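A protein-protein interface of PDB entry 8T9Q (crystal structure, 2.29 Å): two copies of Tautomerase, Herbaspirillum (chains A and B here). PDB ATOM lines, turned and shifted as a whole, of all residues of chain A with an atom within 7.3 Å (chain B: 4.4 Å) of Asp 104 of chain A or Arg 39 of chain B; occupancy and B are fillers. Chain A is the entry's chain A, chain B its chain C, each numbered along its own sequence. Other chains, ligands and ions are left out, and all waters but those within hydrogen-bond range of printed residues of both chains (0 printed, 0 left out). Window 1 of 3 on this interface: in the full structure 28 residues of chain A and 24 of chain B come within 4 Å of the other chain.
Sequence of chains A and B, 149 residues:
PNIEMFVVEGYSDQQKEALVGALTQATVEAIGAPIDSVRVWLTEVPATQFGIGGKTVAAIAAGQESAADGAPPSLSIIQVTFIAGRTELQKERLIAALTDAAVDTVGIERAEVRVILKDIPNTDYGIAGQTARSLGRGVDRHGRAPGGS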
ATOM      1  N   GLU A   4      17.323  11.977 -24.862  1.00  0.00           N
ATOM      2  CA  GLU A   4      16.906  11.324 -26.123  1.00  0.00           C
ATOM      3  C   GLU A   4      16.199  10.033 -25.720  1.00  0.00           C
ATOM      4  O   GLU A   4      16.817   9.204 -25.007  1.00  0.00           O
ATOM      5  CB  GLU A   4      18.093  11.124 -27.064  1.00  0.00           C
ATOM      6  CG  GLU A   4      19.379  10.725 -26.367  1.00  0.00           C
ATOM      7  CD  GLU A   4      20.666  11.093 -27.086  1.00  0.00           C
ATOM      8  OE1 GLU A   4      20.603  11.420 -28.292  1.00  0.00           O
ATOM      9  OE2 GLU A   4      21.735  11.057 -26.433  1.00  0.00           O
ATOM     10  N   MET A   5      14.915   9.933 -26.060  1.00  0.00           N
ATOM     11  CA  MET A   5      14.159   8.673 -25.923  1.00  0.00           C
ATOM     12  C   MET A   5      14.058   8.027 -27.296  1.00  0.00           C
ATOM     13  O   MET A   5      13.487   8.661 -28.205  1.00  0.00           O
ATOM     14  CB  MET A   5      12.752   8.918 -25.384  1.00  0.00           C
ATOM     15  CG  MET A   5      12.072   7.648 -24.915  1.00  0.00           C
ATOM     16  SD  MET A   5      10.363   7.976 -24.483  1.00  0.00           S
ATOM     17  CE  MET A   5      10.178   6.918 -23.046  1.00  0.00           C
ATOM     18  N   PHE A   6      14.533   6.798 -27.437  1.00  0.00           N
ATOM     19  CA  PHE A   6      14.300   6.009 -28.666  1.00  0.00           C
ATOM     20  C   PHE A   6      13.157   5.053 -28.396  1.00  0.00           C
ATOM     21  O   PHE A   6      13.157   4.391 -27.346  1.00  0.00           O
ATOM     22  CB  PHE A   6      15.567   5.302 -29.115  1.00  0.00           C
ATOM     23  CG  PHE A   6      16.801   6.151 -29.078  1.00  0.00           C
ATOM     24  CD1 PHE A   6      17.337   6.577 -27.875  1.00  0.00           C
ATOM     25  CD2 PHE A   6      17.481   6.460 -30.244  1.00  0.00           C
ATOM     26  CE1 PHE A   6      18.503   7.325 -27.838  1.00  0.00           C
ATOM     27  CE2 PHE A   6      18.641   7.214 -30.209  1.00  0.00           C
ATOM     28  CZ  PHE A   6      19.147   7.645 -29.015  1.00  0.00           C
ATOM     29  N   PHE A  50      13.977  -2.064 -35.403  1.00  0.00           N
ATOM     30  CA  PHE A  50      14.165  -2.147 -33.931  1.00  0.00           C
ATOM     31  C   PHE A  50      14.108  -3.615 -33.515  1.00  0.00           C
ATOM     32  O   PHE A  50      13.062  -4.272 -33.708  1.00  0.00           O
ATOM     33  CB  PHE A  50      13.145  -1.243 -33.231  1.00  0.00           C
ATOM     34  CG  PHE A  50      13.524  -0.744 -31.852  1.00  0.00           C
ATOM     35  CD1 PHE A  50      14.680  -1.150 -31.200  1.00  0.00           C
ATOM     36  CD2 PHE A  50      12.688   0.151 -31.191  1.00  0.00           C
ATOM     37  CE1 PHE A  50      15.005  -0.644 -29.947  1.00  0.00           C
ATOM     38  CE2 PHE A  50      12.995   0.632 -29.926  1.00  0.00           C
ATOM     39  CZ  PHE A  50      14.168   0.251 -29.313  1.00  0.00           C
ATOM     40  N   GLY A  51      15.226  -4.148 -33.022  1.00  0.00           N
ATOM     41  CA  GLY A  51      15.366  -5.603 -32.781  1.00  0.00           C
ATOM     42  C   GLY A  51      15.508  -5.947 -31.306  1.00  0.00           C
ATOM     43  O   GLY A  51      16.332  -5.289 -30.649  1.00  0.00           O
ATOM     44  N   ILE A  52      14.781  -6.965 -30.818  1.00  0.00           N
ATOM     45  CA  ILE A  52      14.873  -7.490 -29.413  1.00  0.00           C
ATOM     46  C   ILE A  52      15.254  -8.975 -29.451  1.00  0.00           C
ATOM     47  O   ILE A  52      14.514  -9.778 -30.034  1.00  0.00           O
ATOM     48  CB  ILE A  52      13.569  -7.289 -28.614  1.00  0.00           C
ATOM     49  CG1 ILE A  52      13.689  -7.885 -27.206  1.00  0.00           C
ATOM     50  CG2 ILE A  52      12.355  -7.850 -29.353  1.00  0.00           C
ATOM     51  CD1 ILE A  52      14.781  -7.255 -26.356  1.00  0.00           C
ATOM     52  N   GLY A  53      16.364  -9.341 -28.818  1.00  0.00           N
ATOM     53  CA  GLY A  53      16.864 -10.723 -28.844  1.00  0.00           C
ATOM     54  C   GLY A  53      16.877 -11.328 -30.236  1.00  0.00           C
ATOM     55  O   GLY A  53      16.860 -12.578 -30.349  1.00  0.00           O
ATOM     56  N   GLY A  54      16.977 -10.490 -31.271  1.00  0.00           N
ATOM     57  CA  GLY A  54      17.434 -10.884 -32.614  1.00  0.00           C
ATOM     58  C   GLY A  54      16.352 -10.804 -33.660  1.00  0.00           C
ATOM     59  O   GLY A  54      16.678 -11.041 -34.825  1.00  0.00           O
ATOM     60  N   GLU A  65       9.516   0.031 -27.774  1.00  0.00           N
ATOM     61  CA  GLU A  65      10.276  -0.249 -26.527  1.00  0.00           C
ATOM     62  C   GLU A  65      11.255   0.897 -26.264  1.00  0.00           C
ATOM     63  O   GLU A  65      11.991   1.252 -27.201  1.00  0.00           O
ATOM     64  CB  GLU A  65      11.033  -1.565 -26.662  1.00  0.00           C
ATOM     65  CG  GLU A  65      11.404  -2.158 -25.322  1.00  0.00           C
ATOM     66  CD  GLU A  65      11.717  -3.642 -25.378  1.00  0.00           C
ATOM     67  OE1 GLU A  65      12.414  -4.047 -26.328  1.00  0.00           O
ATOM     68  OE2 GLU A  65      11.253  -4.390 -24.483  1.00  0.00           O
ATOM     69  N   SER A  66      11.274   1.422 -25.030  1.00  0.00           N
ATOM     70  CA  SER A  66      11.823   2.761 -24.688  1.00  0.00           C
ATOM     71  C   SER A  66      13.243   2.644 -24.131  1.00  0.00           C
ATOM     72  O   SER A  66      13.461   1.804 -23.223  1.00  0.00           O
ATOM     73  CB  SER A  66      10.911   3.460 -23.724  1.00  0.00           C
ATOM     74  OG  SER A  66       9.585   3.493 -24.235  1.00  0.00           O
ATOM     75  N   ALA A  67      14.175   3.439 -24.673  1.00  0.00           N
ATOM     76  CA  ALA A  67      15.541   3.617 -24.148  1.00  0.00           C
ATOM     77  C   ALA A  67      15.838   5.112 -24.010  1.00  0.00           C
ATOM     78  O   ALA A  67      15.828   5.833 -25.047  1.00  0.00           O
ATOM     79  CB  ALA A  67      16.522   2.948 -25.059  1.00  0.00           C
ATOM     80  N   ALA A  68      16.143   5.581 -22.802  1.00  0.00           N
ATOM     81  CA  ALA A  68      16.179   7.034 -22.499  1.00  0.00           C
ATOM     82  C   ALA A  68      17.596   7.460 -22.133  1.00  0.00           C
ATOM     83  O   ALA A  68      18.019   7.128 -21.023  1.00  0.00           O
ATOM     84  CB  ALA A  68      15.190   7.366 -21.401  1.00  0.00           C
ATOM     85  N   ASP A  69      18.280   8.204 -23.020  1.00  0.00           N
ATOM     86  CA  ASP A  69      19.651   8.706 -22.748  1.00  0.00           C
ATOM     87  C   ASP A  69      19.545  10.092 -22.111  1.00  0.00           C
ATOM     88  O   ASP A  69      18.957  11.001 -22.730  1.00  0.00           O
ATOM     89  CB  ASP A  69      20.529   8.791 -23.994  1.00  0.00           C
ATOM     90  CG  ASP A  69      20.900   7.463 -24.639  1.00  0.00           C
ATOM     91  OD1 ASP A  69      20.384   6.388 -24.175  1.00  0.00           O
ATOM     92  OD2 ASP A  69      21.669   7.525 -25.642  1.00  0.00           O
ATOM     93  N   GLY A  85      16.822   8.251 -12.520  1.00  0.00           N
ATOM     94  CA  GLY A  85      16.464   6.928 -13.068  1.00  0.00           C
ATOM     95  C   GLY A  85      14.990   6.618 -12.863  1.00  0.00           C
ATOM     96  O   GLY A  85      14.355   6.109 -13.812  1.00  0.00           O
ATOM     97  N   LEU A  89      11.751   6.986 -15.311  1.00  0.00           N
ATOM     98  CA  LEU A  89      11.078   5.703 -15.588  1.00  0.00           C
ATOM     99  C   LEU A  89       9.574   5.861 -15.406  1.00  0.00           C
ATOM    100  O   LEU A  89       8.851   5.469 -16.313  1.00  0.00           O
ATOM    101  CB  LEU A  89      11.590   4.580 -14.707  1.00  0.00           C
ATOM    102  CG  LEU A  89      11.545   3.265 -15.468  1.00  0.00           C
ATOM    103  CD1 LEU A  89      12.819   3.114 -16.284  1.00  0.00           C
ATOM    104  CD2 LEU A  89      11.337   2.085 -14.549  1.00  0.00           C
ATOM    105  N   LEU A  98       3.774   2.196 -21.032  1.00  0.00           N
ATOM    106  CA  LEU A  98       4.539   0.948 -21.267  1.00  0.00           C
ATOM    107  C   LEU A  98       4.826   0.307 -19.908  1.00  0.00           C
ATOM    108  O   LEU A  98       5.014   1.084 -18.940  1.00  0.00           O
ATOM    109  CB  LEU A  98       5.846   1.296 -21.986  1.00  0.00           C
ATOM    110  CG  LEU A  98       6.653   0.081 -22.437  1.00  0.00           C
ATOM    111  CD1 LEU A  98       6.187  -0.388 -23.807  1.00  0.00           C
ATOM    112  CD2 LEU A  98       8.142   0.371 -22.433  1.00  0.00           C
ATOM    113  N   THR A  99       4.865  -1.030 -19.837  1.00  0.00           N
ATOM    114  CA  THR A  99       5.278  -1.784 -18.622  1.00  0.00           C
ATOM    115  C   THR A  99       6.725  -1.409 -18.303  1.00  0.00           C
ATOM    116  O   THR A  99       7.538  -1.290 -19.247  1.00  0.00           O
ATOM    117  CB  THR A  99       5.101  -3.305 -18.767  1.00  0.00           C
ATOM    118  OG1 THR A  99       3.814  -3.576 -19.332  1.00  0.00           O
ATOM    119  CG2 THR A  99       5.241  -4.044 -17.449  1.00  0.00           C
ATOM    120  N   ASP A 100       7.010  -1.199 -17.018  1.00  0.00           N
ATOM    121  CA  ASP A 100       8.329  -0.754 -16.499  1.00  0.00           C
ATOM    122  C   ASP A 100       9.412  -1.707 -17.014  1.00  0.00           C
ATOM    123  O   ASP A 100      10.528  -1.240 -17.291  1.00  0.00           O
ATOM    124  CB  ASP A 100       8.293  -0.660 -14.967  1.00  0.00           C
ATOM    125  CG  ASP A 100       7.235   0.301 -14.442  1.00  0.00           C
ATOM    126  OD1 ASP A 100       6.537   0.922 -15.276  1.00  0.00           O
ATOM    127  OD2 ASP A 100       7.109   0.426 -13.208  1.00  0.00           O
ATOM    128  N   ALA A 101       9.094  -2.997 -17.143  1.00  0.00           N
ATOM    129  CA  ALA A 101      10.054  -4.051 -17.547  1.00  0.00           C
ATOM    130  C   ALA A 101      10.777  -3.650 -18.843  1.00  0.00           C
ATOM    131  O   ALA A 101      11.974  -3.961 -18.970  1.00  0.00           O
ATOM    132  CB  ALA A 101       9.324  -5.367 -17.694  1.00  0.00           C
ATOM    133  N   ALA A 102      10.078  -2.975 -19.763  1.00  0.00           N
ATOM    134  CA  ALA A 102      10.527  -2.691 -21.149  1.00  0.00           C
ATOM    135  C   ALA A 102      11.021  -1.243 -21.279  1.00  0.00           C
ATOM    136  O   ALA A 102      11.031  -0.709 -22.422  1.00  0.00           O
ATOM    137  CB  ALA A 102       9.390  -2.979 -22.095  1.00  0.00           C
ATOM    138  N   VAL A 103      11.484  -0.636 -20.185  1.00  0.00           N
ATOM    139  CA  VAL A 103      12.136   0.697 -20.262  1.00  0.00           C
ATOM    140  C   VAL A 103      13.498   0.645 -19.573  1.00  0.00           C
ATOM    141  O   VAL A 103      13.572   0.249 -18.406  1.00  0.00           O
ATOM    142  CB  VAL A 103      11.233   1.800 -19.687  1.00  0.00           C
ATOM    143  CG1 VAL A 103      10.656   1.410 -18.337  1.00  0.00           C
ATOM    144  CG2 VAL A 103      11.954   3.138 -19.622  1.00  0.00           C
ATOM    145  N   ASP A 104      14.543   1.032 -20.302  1.00  0.00           N
ATOM    146  CA  ASP A 104      15.899   1.241 -19.752  1.00  0.00           C
ATOM    147  C   ASP A 104      16.206   2.748 -19.782  1.00  0.00           C
ATOM    148  O   ASP A 104      15.845   3.429 -20.743  1.00  0.00           O
ATOM    149  CB  ASP A 104      16.917   0.397 -20.513  1.00  0.00           C
ATOM    150  CG  ASP A 104      16.432  -1.012 -20.798  1.00  0.00           C
ATOM    151  OD1 ASP A 104      15.863  -1.637 -19.867  1.00  0.00           O
ATOM    152  OD2 ASP A 104      16.631  -1.484 -21.942  1.00  0.00           O
ATOM    153  N   THR A 105      16.845   3.261 -18.736  1.00  0.00           N
ATOM    154  CA  THR A 105      17.354   4.644 -18.705  1.00  0.00           C
ATOM    155  C   THR A 105      18.869   4.580 -18.628  1.00  0.00           C
ATOM    156  O   THR A 105      19.365   3.690 -17.967  1.00  0.00           O
ATOM    157  CB  THR A 105      16.746   5.442 -17.557  1.00  0.00           C
ATOM    158  OG1 THR A 105      15.379   5.622 -17.927  1.00  0.00           O
ATOM    159  CG2 THR A 105      17.456   6.762 -17.335  1.00  0.00           C
ATOM    160  N   VAL A 106      19.532   5.502 -19.319  1.00  0.00           N
ATOM    161  CA  VAL A 106      21.002   5.565 -19.472  1.00  0.00           C
ATOM    162  C   VAL A 106      21.416   6.962 -19.008  1.00  0.00           C
ATOM    163  O   VAL A 106      20.840   7.984 -19.486  1.00  0.00           O
ATOM    164  CB  VAL A 106      21.396   5.254 -20.928  1.00  0.00           C
ATOM    165  CG1 VAL A 106      22.821   5.667 -21.249  1.00  0.00           C
ATOM    166  CG2 VAL A 106      21.176   3.787 -21.258  1.00  0.00           C
ATOM    167  N   PRO B   1      24.328  -4.647 -25.244  1.00  0.00           N
ATOM    168  CA  PRO B   1      22.887  -4.671 -24.981  1.00  0.00           C
ATOM    169  C   PRO B   1      22.090  -3.428 -25.418  1.00  0.00           C
ATOM    170  O   PRO B   1      20.884  -3.532 -25.428  1.00  0.00           O
ATOM    171  CB  PRO B   1      22.861  -4.842 -23.463  1.00  0.00           C
ATOM    172  CG  PRO B   1      23.998  -5.787 -23.226  1.00  0.00           C
ATOM    173  CD  PRO B   1      25.072  -5.199 -24.115  1.00  0.00           C
ATOM    174  N   ASN B   2      22.747  -2.314 -25.765  1.00  0.00           N
ATOM    175  CA  ASN B   2      22.115  -1.221 -26.567  1.00  0.00           C
ATOM    176  C   ASN B   2      23.007  -0.876 -27.759  1.00  0.00           C
ATOM    177  O   ASN B   2      24.096  -0.313 -27.558  1.00  0.00           O
ATOM    178  CB  ASN B   2      21.801   0.016 -25.738  1.00  0.00           C
ATOM    179  CG  ASN B   2      20.646  -0.241 -24.794  1.00  0.00           C
ATOM    180  OD1 ASN B   2      19.491  -0.296 -25.211  1.00  0.00           O
ATOM    181  ND2 ASN B   2      20.959  -0.431 -23.525  1.00  0.00           N
ATOM    182  N   ILE B   3      22.561  -1.292 -28.939  1.00  0.00           N
ATOM    183  CA  ILE B   3      23.368  -1.304 -30.189  1.00  0.00           C
ATOM    184  C   ILE B   3      22.607  -0.420 -31.171  1.00  0.00           C
ATOM    185  O   ILE B   3      21.473  -0.787 -31.562  1.00  0.00           O
ATOM    186  CB  ILE B   3      23.590  -2.739 -30.714  1.00  0.00           C
ATOM    187  CG1 ILE B   3      24.300  -3.619 -29.687  1.00  0.00           C
ATOM    188  CG2 ILE B   3      24.336  -2.769 -32.036  1.00  0.00           C
ATOM    189  CD1 ILE B   3      24.194  -5.082 -30.013  1.00  0.00           C
ATOM    190  N   SER B  37      18.352  -9.775 -23.461  1.00  0.00           N
ATOM    191  CA  SER B  37      18.983  -8.505 -22.999  1.00  0.00           C
ATOM    192  C   SER B  37      19.422  -7.627 -24.184  1.00  0.00           C
ATOM    193  O   SER B  37      19.810  -6.482 -23.920  1.00  0.00           O
ATOM    194  CB  SER B  37      20.171  -8.752 -22.080  1.00  0.00           C
ATOM    195  OG  SER B  37      19.849  -8.527 -20.715  1.00  0.00           O
ATOM    196  N   VAL B  38      19.389  -8.127 -25.425  1.00  0.00           N
ATOM    197  CA  VAL B  38      20.047  -7.437 -26.571  1.00  0.00           C
ATOM    198  C   VAL B  38      18.989  -6.655 -27.365  1.00  0.00           C
ATOM    199  O   VAL B  38      18.083  -7.268 -27.982  1.00  0.00           O
ATOM    200  CB  VAL B  38      20.842  -8.401 -27.465  1.00  0.00           C
ATOM    201  CG1 VAL B  38      21.676  -7.632 -28.471  1.00  0.00           C
ATOM    202  CG2 VAL B  38      21.733  -9.327 -26.660  1.00  0.00           C
ATOM    203  N   ARG B  39      19.082  -5.331 -27.306  1.00  0.00           N
ATOM    204  CA  ARG B  39      18.238  -4.435 -28.119  1.00  0.00           C
ATOM    205  C   ARG B  39      19.148  -3.799 -29.173  1.00  0.00           C
ATOM    206  O   ARG B  39      20.232  -3.332 -28.820  1.00  0.00           O
ATOM    207  CB  ARG B  39      17.540  -3.387 -27.255  1.00  0.00           C
ATOM    208  CG  ARG B  39      16.799  -3.906 -26.033  1.00  0.00           C
ATOM    209  CD  ARG B  39      16.020  -2.720 -25.466  1.00  0.00           C
ATOM    210  NE  ARG B  39      15.152  -2.932 -24.309  1.00  0.00           N
ATOM    211  CZ  ARG B  39      14.443  -1.965 -23.707  1.00  0.00           C
ATOM    212  NH1 ARG B  39      14.499  -0.713 -24.141  1.00  0.00           N
ATOM    213  NH2 ARG B  39      13.691  -2.245 -22.657  1.00  0.00           N
ATOM    214  N   VAL B  40      18.750  -3.869 -30.434  1.00  0.00           N
ATOM    215  CA  VAL B  40      19.576  -3.387 -31.576  1.00  0.00           C
ATOM    216  C   VAL B  40      18.691  -2.426 -32.346  1.00  0.00           C
ATOM    217  O   VAL B  40      17.565  -2.850 -32.670  1.00  0.00           O
ATOM    218  CB  VAL B  40      20.051  -4.538 -32.475  1.00  0.00           C
ATOM    219  CG1 VAL B  40      20.908  -4.012 -33.638  1.00  0.00           C
ATOM    220  CG2 VAL B  40      20.802  -5.595 -31.679  1.00  0.00           C
ATOM    221  N   TRP B  41      19.125  -1.187 -32.592  1.00  0.00           N
ATOM    222  CA  TRP B  41      18.337  -0.344 -33.555  1.00  0.00           C
ATOM    223  C   TRP B  41      19.228   0.210 -34.658  1.00  0.00           C
ATOM    224  O   TRP B  41      20.394   0.609 -34.418  1.00  0.00           O
ATOM    225  CB  TRP B  41      17.473   0.743 -32.883  1.00  0.00           C
ATOM    226  CG  TRP B  41      18.158   1.708 -31.975  1.00  0.00           C
ATOM    227  CD1 TRP B  41      18.484   3.005 -32.266  1.00  0.00           C
ATOM    228  CD2 TRP B  41      18.480   1.516 -30.586  1.00  0.00           C
ATOM    229  NE1 TRP B  41      19.041   3.611 -31.171  1.00  0.00           N
ATOM    230  CE2 TRP B  41      19.066   2.717 -30.132  1.00  0.00           C
ATOM    231  CE3 TRP B  41      18.380   0.441 -29.698  1.00  0.00           C
ATOM    232  CZ2 TRP B  41      19.557   2.858 -28.836  1.00  0.00           C
ATOM    233  CZ3 TRP B  41      18.875   0.575 -28.427  1.00  0.00           C
ATOM    234  CH2 TRP B  41      19.439   1.775 -27.997  1.00  0.00           C
ATOM    235  N   ILE B 116      19.632   2.353 -15.535  1.00  0.00           N
ATOM    236  CA  ILE B 116      18.349   1.970 -14.882  1.00  0.00           C
ATOM    237  C   ILE B 116      17.585   0.988 -15.789  1.00  0.00           C
ATOM    238  O   ILE B 116      17.132   1.387 -16.883  1.00  0.00           O
ATOM    239  CB  ILE B 116      17.584   3.242 -14.449  1.00  0.00           C
ATOM    240  CG1 ILE B 116      17.907   3.611 -12.997  1.00  0.00           C
ATOM    241  CG2 ILE B 116      16.081   3.114 -14.662  1.00  0.00           C
ATOM    242  CD1 ILE B 116      19.101   4.537 -12.819  1.00  0.00           C
ATOM    243  N   LEU B 117      17.495  -0.277 -15.356  1.00  0.00           N
ATOM    244  CA  LEU B 117      16.711  -1.355 -16.026  1.00  0.00           C
ATOM    245  C   LEU B 117      15.509  -1.688 -15.132  1.00  0.00           C
ATOM    246  O   LEU B 117      15.726  -2.041 -13.941  1.00  0.00           O
ATOM    247  CB  LEU B 117      17.611  -2.567 -16.312  1.00  0.00           C
ATOM    248  CG  LEU B 117      17.926  -3.521 -15.156  1.00  0.00           C
ATOM    249  CD1 LEU B 117      18.537  -4.816 -15.678  1.00  0.00           C
ATOM    250  CD2 LEU B 117      18.853  -2.882 -14.130  1.00  0.00           C
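The backbone carbonyl oxygen of Ala 67 of chain A lies within hydrogen-bond range of the backbone NH of Phe 6 of chain A (2.9 Å). The backbone carbonyl oxygen of Ala 102 of chain A sits at hydrogen-bond distance from the backbone NH of Ser 66 of chain A (3.4 Å). The backbone NH of Asp 104 of chain A sits at hydrogen-bond distance from the backbone carbonyl oxygen of Ser 66 of chain A (3.2 Å). The backbone NH of Ala 68 of chain A sits at hydrogen-bond distance from the backbone carbonyl oxygen of Asp 104 of chain A. N of Ile 3 of chain B lies within hydrogen-bond range of O of Arg 39 of chain B, at 3.1 Å. The backbone NH (N) of Trp 41 of chain B lies within hydrogen-bond range of the backbone carbonyl oxygen (O) of Ile 3 of chain B (2.6 Å).
No position is printed for both chains. Of the 19 pairs that touch across the chains among the printed residues, none has its exchanged pair printed and touching as well.
The backbone carbonyl oxygen (O) of Val 40 of chain B sits at hydrogen-bond distance from the backbone NH (N) of Gly 51 of chain A (2.7 Å). The backbone NH of Gly 53 of chain A sits at hydrogen-bond distance from the backbone carbonyl oxygen of Val 38 of chain B, 2.8 Å away. OE1 of Glu 65 of chain A lies within salt-bridge range of NE of Arg 39 of chain B, at 3.6 Å. NH1 of Arg 39 of chain B sits at hydrogen-bond distance from O of Ser 66 of chain A. The guanidinium group (NH2) of Arg 39 of chain B is in hydrogen-bond range of the backbone carbonyl oxygen (O) of Ala 102 of chain A, at 3.1 Å. OD2 of Asp 104 of chain A lies within salt-bridge range of NH2 of Arg 39 of chain B (3.1 Å). The backbone NH of Thr 105 of chain A is in hydrogen-bond range of the backbone carbonyl oxygen of Ile 116 of chain B (2.7 Å).
Met 5 of chain A touches none of the printed residues of chain B. Of the printed residues of chain B, Leu 89 of chain A touches Ile 116. Asp 100 of chain A touches none of the printed residues of chain B. Of the printed residues of chain B, Val 103 of chain A touches Arg 39 (3.7 Å). Asp 104 of chain A touches just these residues of chain B: Arg 39, Ile 116 and Leu 117. Arg 39 of chain B touches seven residues of chain A. Of the printed residues of chain A, Val 40 of chain B touches Phe 50 (3.6 Å) and Gly 51 (2.7 Å). Of the printed residues of chain A, Ile 116 of chain B touches Gly 85, Leu 89, Asp 104 and Thr 105. The nearest residue of chain A that does not touch Arg 39 of chain B is Ala 67 of chain A (4.2 Å). The nearest printed residue of chain A that does not touch Val 40 of chain B is Ile 52 of chain A (5.0 Å).
Hydrophobic or aromatic side chains of chain B within 4 Å of the printed part of chain A: Trp 41 and Ile 116. Along chain B the printed residues that touch a printed residue of chain A span positions 38 to 117. Of the 24 printed residues of chain A, 13 touch a printed residue of chain B. Among the printed residues, 19 pairs touch across the chains.
CD2 of Phe 6 of chain A touches NE1 of Trp 41 of chain B, 3.4 Å away. Phe 50 of chain A touches Val 40 of chain B (C to O, 3.6 Å). CE1 of Phe 50 of chain A touches CE3 of Trp 41 of chain B, 3.6 Å away. Gly 51 of chain A touches Val 38 of chain B (O to O, 3.8 Å). Arg 39 of chain B touches Gly 51 of chain A. Val 38 of chain B touches Ile 52 of chain A. Arg 39 of chain B touches Ile 52 of chain A (CG to CD1, 3.9 Å). Gly 85 of chain A touches Ile 116 of chain B (O to CG2, 3.6 Å). CD1 of Leu 89 of chain A touches CG2 of Ile 116 of chain B, at 3.6 Å. N of Val 103 of chain A touches NH2 of Arg 39 of chain B, 3.7 Å away.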
